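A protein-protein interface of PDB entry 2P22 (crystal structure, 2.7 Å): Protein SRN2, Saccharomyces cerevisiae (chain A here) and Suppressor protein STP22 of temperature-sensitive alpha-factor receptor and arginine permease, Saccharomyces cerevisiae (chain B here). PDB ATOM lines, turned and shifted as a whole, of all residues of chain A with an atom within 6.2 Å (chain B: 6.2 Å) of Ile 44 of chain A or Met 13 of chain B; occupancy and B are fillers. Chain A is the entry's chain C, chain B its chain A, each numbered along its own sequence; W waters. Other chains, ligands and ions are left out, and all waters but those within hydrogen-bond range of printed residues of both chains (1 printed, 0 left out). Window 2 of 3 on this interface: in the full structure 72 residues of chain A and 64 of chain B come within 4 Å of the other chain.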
ATOM      1  N   LEU A  37       7.948  -4.572  -1.367  1.00  0.00           N
ATOM      2  CA  LEU A  37       6.725  -4.810  -2.128  1.00  0.00           C
ATOM      3  C   LEU A  37       6.964  -5.574  -3.426  1.00  0.00           C
ATOM      4  O   LEU A  37       7.990  -5.396  -4.098  1.00  0.00           O
ATOM      5  CB  LEU A  37       5.997  -3.495  -2.428  1.00  0.00           C
ATOM      6  CG  LEU A  37       4.753  -3.266  -1.568  1.00  0.00           C
ATOM      7  CD1 LEU A  37       5.167  -2.950  -0.137  1.00  0.00           C
ATOM      8  CD2 LEU A  37       3.945  -2.139  -2.156  1.00  0.00           C
ATOM      9  N   SER A  39       7.321  -7.596  -6.891  1.00  0.00           N
ATOM     10  CA  SER A  39       8.083  -7.260  -8.089  1.00  0.00           C
ATOM     11  C   SER A  39       7.526  -6.008  -8.782  1.00  0.00           C
ATOM     12  O   SER A  39       8.247  -5.302  -9.496  1.00  0.00           O
ATOM     13  CB  SER A  39       8.082  -8.464  -9.050  1.00  0.00           C
ATOM     14  OG  SER A  39       8.941  -8.249 -10.159  1.00  0.00           O
ATOM     15  N   SER A  40       6.246  -5.733  -8.550  1.00  0.00           N
ATOM     16  CA  SER A  40       5.597  -4.580  -9.139  1.00  0.00           C
ATOM     17  C   SER A  40       4.086  -4.601  -8.910  1.00  0.00           C
ATOM     18  O   SER A  40       3.469  -3.557  -8.713  1.00  0.00           O
ATOM     19  CB  SER A  40       5.908  -4.528 -10.638  1.00  0.00           C
ATOM     20  OG  SER A  40       6.010  -5.836 -11.186  1.00  0.00           O
ATOM     21  N   LYS A  41       3.498  -5.794  -8.924  1.00  0.00           N
ATOM     22  CA  LYS A  41       2.060  -5.944  -8.734  1.00  0.00           C
ATOM     23  C   LYS A  41       1.546  -5.254  -7.472  1.00  0.00           C
ATOM     24  O   LYS A  41       0.377  -4.857  -7.403  1.00  0.00           O
ATOM     25  CB  LYS A  41       1.675  -7.433  -8.723  1.00  0.00           C
ATOM     26  CG  LYS A  41       1.523  -8.050 -10.121  1.00  0.00           C
ATOM     27  CD  LYS A  41       0.440  -7.317 -10.934  1.00  0.00           C
ATOM     28  CE  LYS A  41       0.288  -7.856 -12.357  1.00  0.00           C
ATOM     29  NZ  LYS A  41      -0.764  -7.111 -13.111  1.00  0.00           N
ATOM     30  N   GLU A  42       2.416  -5.102  -6.481  1.00  0.00           N
ATOM     31  CA  GLU A  42       2.029  -4.448  -5.238  1.00  0.00           C
ATOM     32  C   GLU A  42       2.310  -2.938  -5.287  1.00  0.00           C
ATOM     33  O   GLU A  42       1.512  -2.133  -4.800  1.00  0.00           O
ATOM     34  CB  GLU A  42       2.738  -5.112  -4.053  1.00  0.00           C
ATOM     35  CG  GLU A  42       2.139  -6.468  -3.686  1.00  0.00           C
ATOM     36  CD  GLU A  42       2.840  -7.144  -2.506  1.00  0.00           C
ATOM     37  OE1 GLU A  42       4.067  -7.384  -2.590  1.00  0.00           O
ATOM     38  OE2 GLU A  42       2.162  -7.445  -1.495  1.00  0.00           O
ATOM     39  N   ILE A  43       3.432  -2.562  -5.893  1.00  0.00           N
ATOM     40  CA  ILE A  43       3.796  -1.157  -6.035  1.00  0.00           C
ATOM     41  C   ILE A  43       2.753  -0.489  -6.926  1.00  0.00           C
ATOM     42  O   ILE A  43       2.205   0.570  -6.591  1.00  0.00           O
ATOM     43  CB  ILE A  43       5.187  -1.046  -6.659  1.00  0.00           C
ATOM     44  CG1 ILE A  43       6.217  -1.549  -5.638  1.00  0.00           C
ATOM     45  CG2 ILE A  43       5.478   0.375  -7.080  1.00  0.00           C
ATOM     46  CD1 ILE A  43       7.630  -1.512  -6.132  1.00  0.00           C
ATOM     47  N   ILE A  44       2.487  -1.153  -8.053  1.00  0.00           N
ATOM     48  CA  ILE A  44       1.516  -0.749  -9.060  1.00  0.00           C
ATOM     49  C   ILE A  44       0.137  -0.586  -8.433  1.00  0.00           C
ATOM     50  O   ILE A  44      -0.567   0.391  -8.685  1.00  0.00           O
ATOM     51  CB  ILE A  44       1.436  -1.823 -10.176  1.00  0.00           C
ATOM     52  CG1 ILE A  44       2.738  -1.823 -10.976  1.00  0.00           C
ATOM     53  CG2 ILE A  44       0.222  -1.575 -11.084  1.00  0.00           C
ATOM     54  CD1 ILE A  44       2.830  -2.937 -11.992  1.00  0.00           C
ATOM     55  N   ASP A  45      -0.238  -1.567  -7.627  1.00  0.00           N
ATOM     56  CA  ASP A  45      -1.508  -1.564  -6.929  1.00  0.00           C
ATOM     57  C   ASP A  45      -1.493  -0.432  -5.909  1.00  0.00           C
ATOM     58  O   ASP A  45      -2.481   0.287  -5.735  1.00  0.00           O
ATOM     59  CB  ASP A  45      -1.717  -2.929  -6.244  1.00  0.00           C
ATOM     60  CG  ASP A  45      -2.700  -2.874  -5.066  1.00  0.00           C
ATOM     61  OD1 ASP A  45      -2.260  -2.542  -3.937  1.00  0.00           O
ATOM     62  OD2 ASP A  45      -3.907  -3.169  -5.261  1.00  0.00           O
ATOM     63  N   LEU A  46      -0.359  -0.255  -5.242  1.00  0.00           N
ATOM     64  CA  LEU A  46      -0.260   0.788  -4.237  1.00  0.00           C
ATOM     65  C   LEU A  46      -0.409   2.165  -4.873  1.00  0.00           C
ATOM     66  O   LEU A  46      -1.102   3.012  -4.332  1.00  0.00           O
ATOM     67  CB  LEU A  46       1.070   0.648  -3.486  1.00  0.00           C
ATOM     68  CG  LEU A  46       1.469   1.513  -2.279  1.00  0.00           C
ATOM     69  CD1 LEU A  46       2.422   2.583  -2.748  1.00  0.00           C
ATOM     70  CD2 LEU A  46       0.259   2.099  -1.570  1.00  0.00           C
ATOM     71  N   ILE A  47       0.216   2.376  -6.030  1.00  0.00           N
ATOM     72  CA  ILE A  47       0.138   3.657  -6.740  1.00  0.00           C
ATOM     73  C   ILE A  47      -1.170   3.886  -7.502  1.00  0.00           C
ATOM     74  O   ILE A  47      -1.793   4.942  -7.394  1.00  0.00           O
ATOM     75  CB  ILE A  47       1.238   3.793  -7.786  1.00  0.00           C
ATOM     76  CG1 ILE A  47       2.591   3.527  -7.150  1.00  0.00           C
ATOM     77  CG2 ILE A  47       1.163   5.176  -8.427  1.00  0.00           C
ATOM     78  CD1 ILE A  47       3.765   3.766  -8.103  1.00  0.00           C
ATOM     79  N   GLN A  48      -1.562   2.890  -8.285  1.00  0.00           N
ATOM     80  CA  GLN A  48      -2.756   2.978  -9.103  1.00  0.00           C
ATOM     81  C   GLN A  48      -4.075   2.867  -8.374  1.00  0.00           C
ATOM     82  O   GLN A  48      -5.096   3.347  -8.857  1.00  0.00           O
ATOM     83  CB  GLN A  48      -2.705   1.917 -10.188  1.00  0.00           C
ATOM     84  CG  GLN A  48      -1.859   2.313 -11.362  1.00  0.00           C
ATOM     85  CD  GLN A  48      -1.679   1.177 -12.332  1.00  0.00           C
ATOM     86  OE1 GLN A  48      -2.623   0.438 -12.613  1.00  0.00           O
ATOM     87  NE2 GLN A  48      -0.466   1.031 -12.862  1.00  0.00           N
ATOM     88  N   THR A  49      -4.053   2.255  -7.203  1.00  0.00           N
ATOM     89  CA  THR A  49      -5.276   2.057  -6.463  1.00  0.00           C
ATOM     90  C   THR A  49      -5.312   2.705  -5.091  1.00  0.00           C
ATOM     91  O   THR A  49      -6.382   2.851  -4.485  1.00  0.00           O
ATOM     92  CB  THR A  49      -5.536   0.552  -6.335  1.00  0.00           C
ATOM     93  OG1 THR A  49      -5.586  -0.018  -7.647  1.00  0.00           O
ATOM     94  CG2 THR A  49      -6.843   0.278  -5.617  1.00  0.00           C
ATOM     95  N   HIS A  50      -4.158   3.119  -4.591  1.00  0.00           N
ATOM     96  CA  HIS A  50      -4.139   3.728  -3.270  1.00  0.00           C
ATOM     97  C   HIS A  50      -3.477   5.092  -3.208  1.00  0.00           C
ATOM     98  O   HIS A  50      -2.877   5.442  -2.197  1.00  0.00           O
ATOM     99  CB  HIS A  50      -3.487   2.755  -2.292  1.00  0.00           C
ATOM    100  CG  HIS A  50      -4.119   1.400  -2.312  1.00  0.00           C
ATOM    101  ND1 HIS A  50      -5.419   1.185  -1.904  1.00  0.00           N
ATOM    102  CD2 HIS A  50      -3.662   0.208  -2.758  1.00  0.00           C
ATOM    103  CE1 HIS A  50      -5.735  -0.083  -2.101  1.00  0.00           C
ATOM    104  NE2 HIS A  50      -4.687  -0.698  -2.618  1.00  0.00           N
ATOM    105  N   THR B   8      15.292  -3.619 -13.332  1.00  0.00           N
ATOM    106  CA  THR B   8      14.696  -2.504 -14.066  1.00  0.00           C
ATOM    107  C   THR B   8      13.176  -2.447 -13.908  1.00  0.00           C
ATOM    108  O   THR B   8      12.609  -1.365 -13.783  1.00  0.00           O
ATOM    109  CB  THR B   8      15.057  -2.547 -15.582  1.00  0.00           C
ATOM    110  OG1 THR B   8      16.455  -2.285 -15.748  1.00  0.00           O
ATOM    111  CG2 THR B   8      14.266  -1.494 -16.359  1.00  0.00           C
ATOM    112  N   ASN B   9      12.515  -3.602 -13.899  1.00  0.00           N
ATOM    113  CA  ASN B   9      11.062  -3.638 -13.748  1.00  0.00           C
ATOM    114  C   ASN B   9      10.689  -3.078 -12.377  1.00  0.00           C
ATOM    115  O   ASN B   9      10.188  -1.955 -12.262  1.00  0.00           O
ATOM    116  CB  ASN B   9      10.551  -5.077 -13.866  1.00  0.00           C
ATOM    117  CG  ASN B   9       9.032  -5.162 -13.853  1.00  0.00           C
ATOM    118  OD1 ASN B   9       8.458  -6.242 -13.681  1.00  0.00           O
ATOM    119  ND2 ASN B   9       8.374  -4.023 -14.045  1.00  0.00           N
ATOM    120  N   HIS B  10      10.945  -3.886 -11.352  1.00  0.00           N
ATOM    121  CA  HIS B  10      10.692  -3.544  -9.958  1.00  0.00           C
ATOM    122  C   HIS B  10      11.343  -2.209  -9.590  1.00  0.00           C
ATOM    123  O   HIS B  10      10.872  -1.513  -8.691  1.00  0.00           O
ATOM    124  CB  HIS B  10      11.244  -4.654  -9.061  1.00  0.00           C
ATOM    125  CG  HIS B  10      11.065  -4.399  -7.597  1.00  0.00           C
ATOM    126  ND1 HIS B  10      11.935  -3.619  -6.865  1.00  0.00           N
ATOM    127  CD2 HIS B  10      10.102  -4.801  -6.732  1.00  0.00           C
ATOM    128  CE1 HIS B  10      11.516  -3.553  -5.612  1.00  0.00           C
ATOM    129  NE2 HIS B  10      10.405  -4.261  -5.504  1.00  0.00           N
ATOM    130  N   HIS B  11      12.421  -1.859 -10.294  1.00  0.00           N
ATOM    131  CA  HIS B  11      13.153  -0.619 -10.055  1.00  0.00           C
ATOM    132  C   HIS B  11      12.394   0.567 -10.622  1.00  0.00           C
ATOM    133  O   HIS B  11      12.263   1.607  -9.973  1.00  0.00           O
ATOM    134  CB  HIS B  11      14.545  -0.690 -10.697  1.00  0.00           C
ATOM    135  CG  HIS B  11      15.417   0.494 -10.396  1.00  0.00           C
ATOM    136  ND1 HIS B  11      15.821   0.820  -9.118  1.00  0.00           N
ATOM    137  CD2 HIS B  11      15.942   1.445 -11.207  1.00  0.00           C
ATOM    138  CE1 HIS B  11      16.555   1.920  -9.154  1.00  0.00           C
ATOM    139  NE2 HIS B  11      16.642   2.320 -10.411  1.00  0.00           N
ATOM    140  N   GLU B  12      11.886   0.408 -11.837  1.00  0.00           N
ATOM    141  CA  GLU B  12      11.140   1.477 -12.482  1.00  0.00           C
ATOM    142  C   GLU B  12       9.821   1.763 -11.754  1.00  0.00           C
ATOM    143  O   GLU B  12       9.366   2.907 -11.734  1.00  0.00           O
ATOM    144  CB  GLU B  12      10.886   1.116 -13.946  1.00  0.00           C
ATOM    145  CG  GLU B  12      10.181   2.197 -14.740  1.00  0.00           C
ATOM    146  CD  GLU B  12       9.921   1.769 -16.171  1.00  0.00           C
ATOM    147  OE1 GLU B  12       9.208   0.759 -16.378  1.00  0.00           O
ATOM    148  OE2 GLU B  12      10.433   2.442 -17.090  1.00  0.00           O
ATOM    149  N   MET B  13       9.207   0.737 -11.158  1.00  0.00           N
ATOM    150  CA  MET B  13       7.955   0.947 -10.420  1.00  0.00           C
ATOM    151  C   MET B  13       8.260   1.794  -9.196  1.00  0.00           C
ATOM    152  O   MET B  13       7.558   2.769  -8.892  1.00  0.00           O
ATOM    153  CB  MET B  13       7.320  -0.381  -9.978  1.00  0.00           C
ATOM    154  CG  MET B  13       6.732  -1.218 -11.125  1.00  0.00           C
ATOM    155  SD  MET B  13       5.498  -0.345 -12.212  1.00  0.00           S
ATOM    156  CE  MET B  13       6.621   0.715 -13.319  1.00  0.00           C
ATOM    157  N   LEU B  14       9.329   1.412  -8.502  1.00  0.00           N
ATOM    158  CA  LEU B  14       9.773   2.120  -7.309  1.00  0.00           C
ATOM    159  C   LEU B  14      10.147   3.547  -7.716  1.00  0.00           C
ATOM    160  O   LEU B  14       9.966   4.496  -6.955  1.00  0.00           O
ATOM    161  CB  LEU B  14      10.967   1.383  -6.697  1.00  0.00           C
ATOM    162  CG  LEU B  14      10.918   1.008  -5.216  1.00  0.00           C
ATOM    163  CD1 LEU B  14       9.525   0.573  -4.799  1.00  0.00           C
ATOM    164  CD2 LEU B  14      11.913  -0.110  -4.973  1.00  0.00           C
ATOM    165  N   GLN B  15      10.644   3.694  -8.935  1.00  0.00           N
ATOM    166  CA  GLN B  15      11.004   5.002  -9.432  1.00  0.00           C
ATOM    167  C   GLN B  15       9.718   5.817  -9.619  1.00  0.00           C
ATOM    168  O   GLN B  15       9.669   7.006  -9.303  1.00  0.00           O
ATOM    169  CB  GLN B  15      11.743   4.852 -10.752  1.00  0.00           C
ATOM    170  CG  GLN B  15      12.362   6.116 -11.270  1.00  0.00           C
ATOM    171  CD  GLN B  15      12.922   5.920 -12.650  1.00  0.00           C
ATOM    172  OE1 GLN B  15      13.559   4.903 -12.930  1.00  0.00           O
ATOM    173  NE2 GLN B  15      12.695   6.893 -13.526  1.00  0.00           N
ATOM    174  N   ASN B  16       8.672   5.178 -10.132  1.00  0.00           N
ATOM    175  CA  ASN B  16       7.404   5.873 -10.322  1.00  0.00           C
ATOM    176  C   ASN B  16       6.807   6.302  -8.998  1.00  0.00           C
ATOM    177  O   ASN B  16       6.184   7.350  -8.905  1.00  0.00           O
ATOM    178  CB  ASN B  16       6.384   4.984 -11.015  1.00  0.00           C
ATOM    179  CG  ASN B  16       6.493   5.045 -12.508  1.00  0.00           C
ATOM    180  OD1 ASN B  16       6.950   6.054 -13.065  1.00  0.00           O
ATOM    181  ND2 ASN B  16       6.062   3.975 -13.180  1.00  0.00           N
ATOM    182  N   LEU B  17       6.994   5.460  -7.991  1.00  0.00           N
ATOM    183  CA  LEU B  17       6.481   5.708  -6.668  1.00  0.00           C
ATOM    184  C   LEU B  17       7.084   6.952  -6.065  1.00  0.00           C
ATOM    185  O   LEU B  17       6.417   7.706  -5.356  1.00  0.00           O
ATOM    186  CB  LEU B  17       6.791   4.533  -5.765  1.00  0.00           C
ATOM    187  CG  LEU B  17       6.001   4.585  -4.466  1.00  0.00           C
ATOM    188  CD1 LEU B  17       4.513   4.665  -4.802  1.00  0.00           C
ATOM    189  CD2 LEU B  17       6.315   3.345  -3.628  1.00  0.00           C
ATOM    190  N   GLN B  18       8.356   7.160  -6.365  1.00  0.00           N
ATOM    191  CA  GLN B  18       9.100   8.293  -5.852  1.00  0.00           C
ATOM    192  C   GLN B  18       8.535   9.587  -6.419  1.00  0.00           C
ATOM    193  O   GLN B  18       8.269  10.545  -5.683  1.00  0.00           O
ATOM    194  CB  GLN B  18      10.585   8.121  -6.212  1.00  0.00           C
ATOM    195  CG  GLN B  18      11.569   9.125  -5.589  1.00  0.00           C
ATOM    196  CD  GLN B  18      11.607   9.105  -4.071  1.00  0.00           C
ATOM    197  OE1 GLN B  18      10.790   9.738  -3.407  1.00  0.00           O
ATOM    198  NE2 GLN B  18      12.556   8.373  -3.517  1.00  0.00           N
HETATM  199  O   HOH W   1      10.875  -6.974 -10.982  1.00  0.00           O
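O of Leu 37 of chain A lies within hydrogen-bond range of NE2 of His 10 of chain B (3.0 Å).
His 10 of chain B touches Ser 39 of chain A.
Asn 9 of chain B touches Ser 40 of chain A (OD1 to OG, 3.5 Å).
Ser 40 of chain A touches Met 13 of chain B.
His 10 of chain B touches Ile 43 of chain A.
CG2 of Ile 43 of chain A touches CB of Met 13 of chain B (3.5 Å).
CD1 of Ile 43 of chain A touches CD1 of Leu 14 of chain B, 3.1 Å away.
SD of Met 13 of chain B touches CG1 of Ile 44 of chain A, at 3.4 Å.
Leu 46 of chain A touches Leu 17 of chain B (CD1 to CD1, 3.6 Å).
Ile 47 of chain A touches Leu 17 of chain B.
Printed residues of chain B within 4 Å of Ile 43 of chain A: His 10, Met 13 and Leu 14.
Ile 44 of chain A touches just one residue of chain B: Met 13 (3.4 Å).
Printed residues of chain A within 4 Å of His 10 of chain B: Leu 37 (3.0 Å), Ser 39 (3.0 Å) and Ile 43 (3.96 Å).
Printed residues of chain A within 4 Å of Leu 14 of chain B: Ile 43 (3.1 Å).
The nearest printed residue of chain A that does not touch Met 13 of chain B is Ile 47 of chain A (4.0004 Å).
The nearest printed residue of chain A that does not touch Asn 9 of chain B is Ser 39 of chain A (4.1 Å).
Hydrophobic or aromatic side chains of chain B within 4 Å of the printed part of chain A: His 10, Met 13, Leu 14 and Leu 17.
Among the printed residues, 10 pairs touch across the chains.
Among the printed residues, no Asp or Glu carboxylate lies within 4 Å of a Lys or Arg side-chain nitrogen of the other chain.
Water W1 lies within hydrogen-bond range of OG of Ser 39 of chain A (2.5 Å) and N of His 10 of chain B (3.1 Å).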
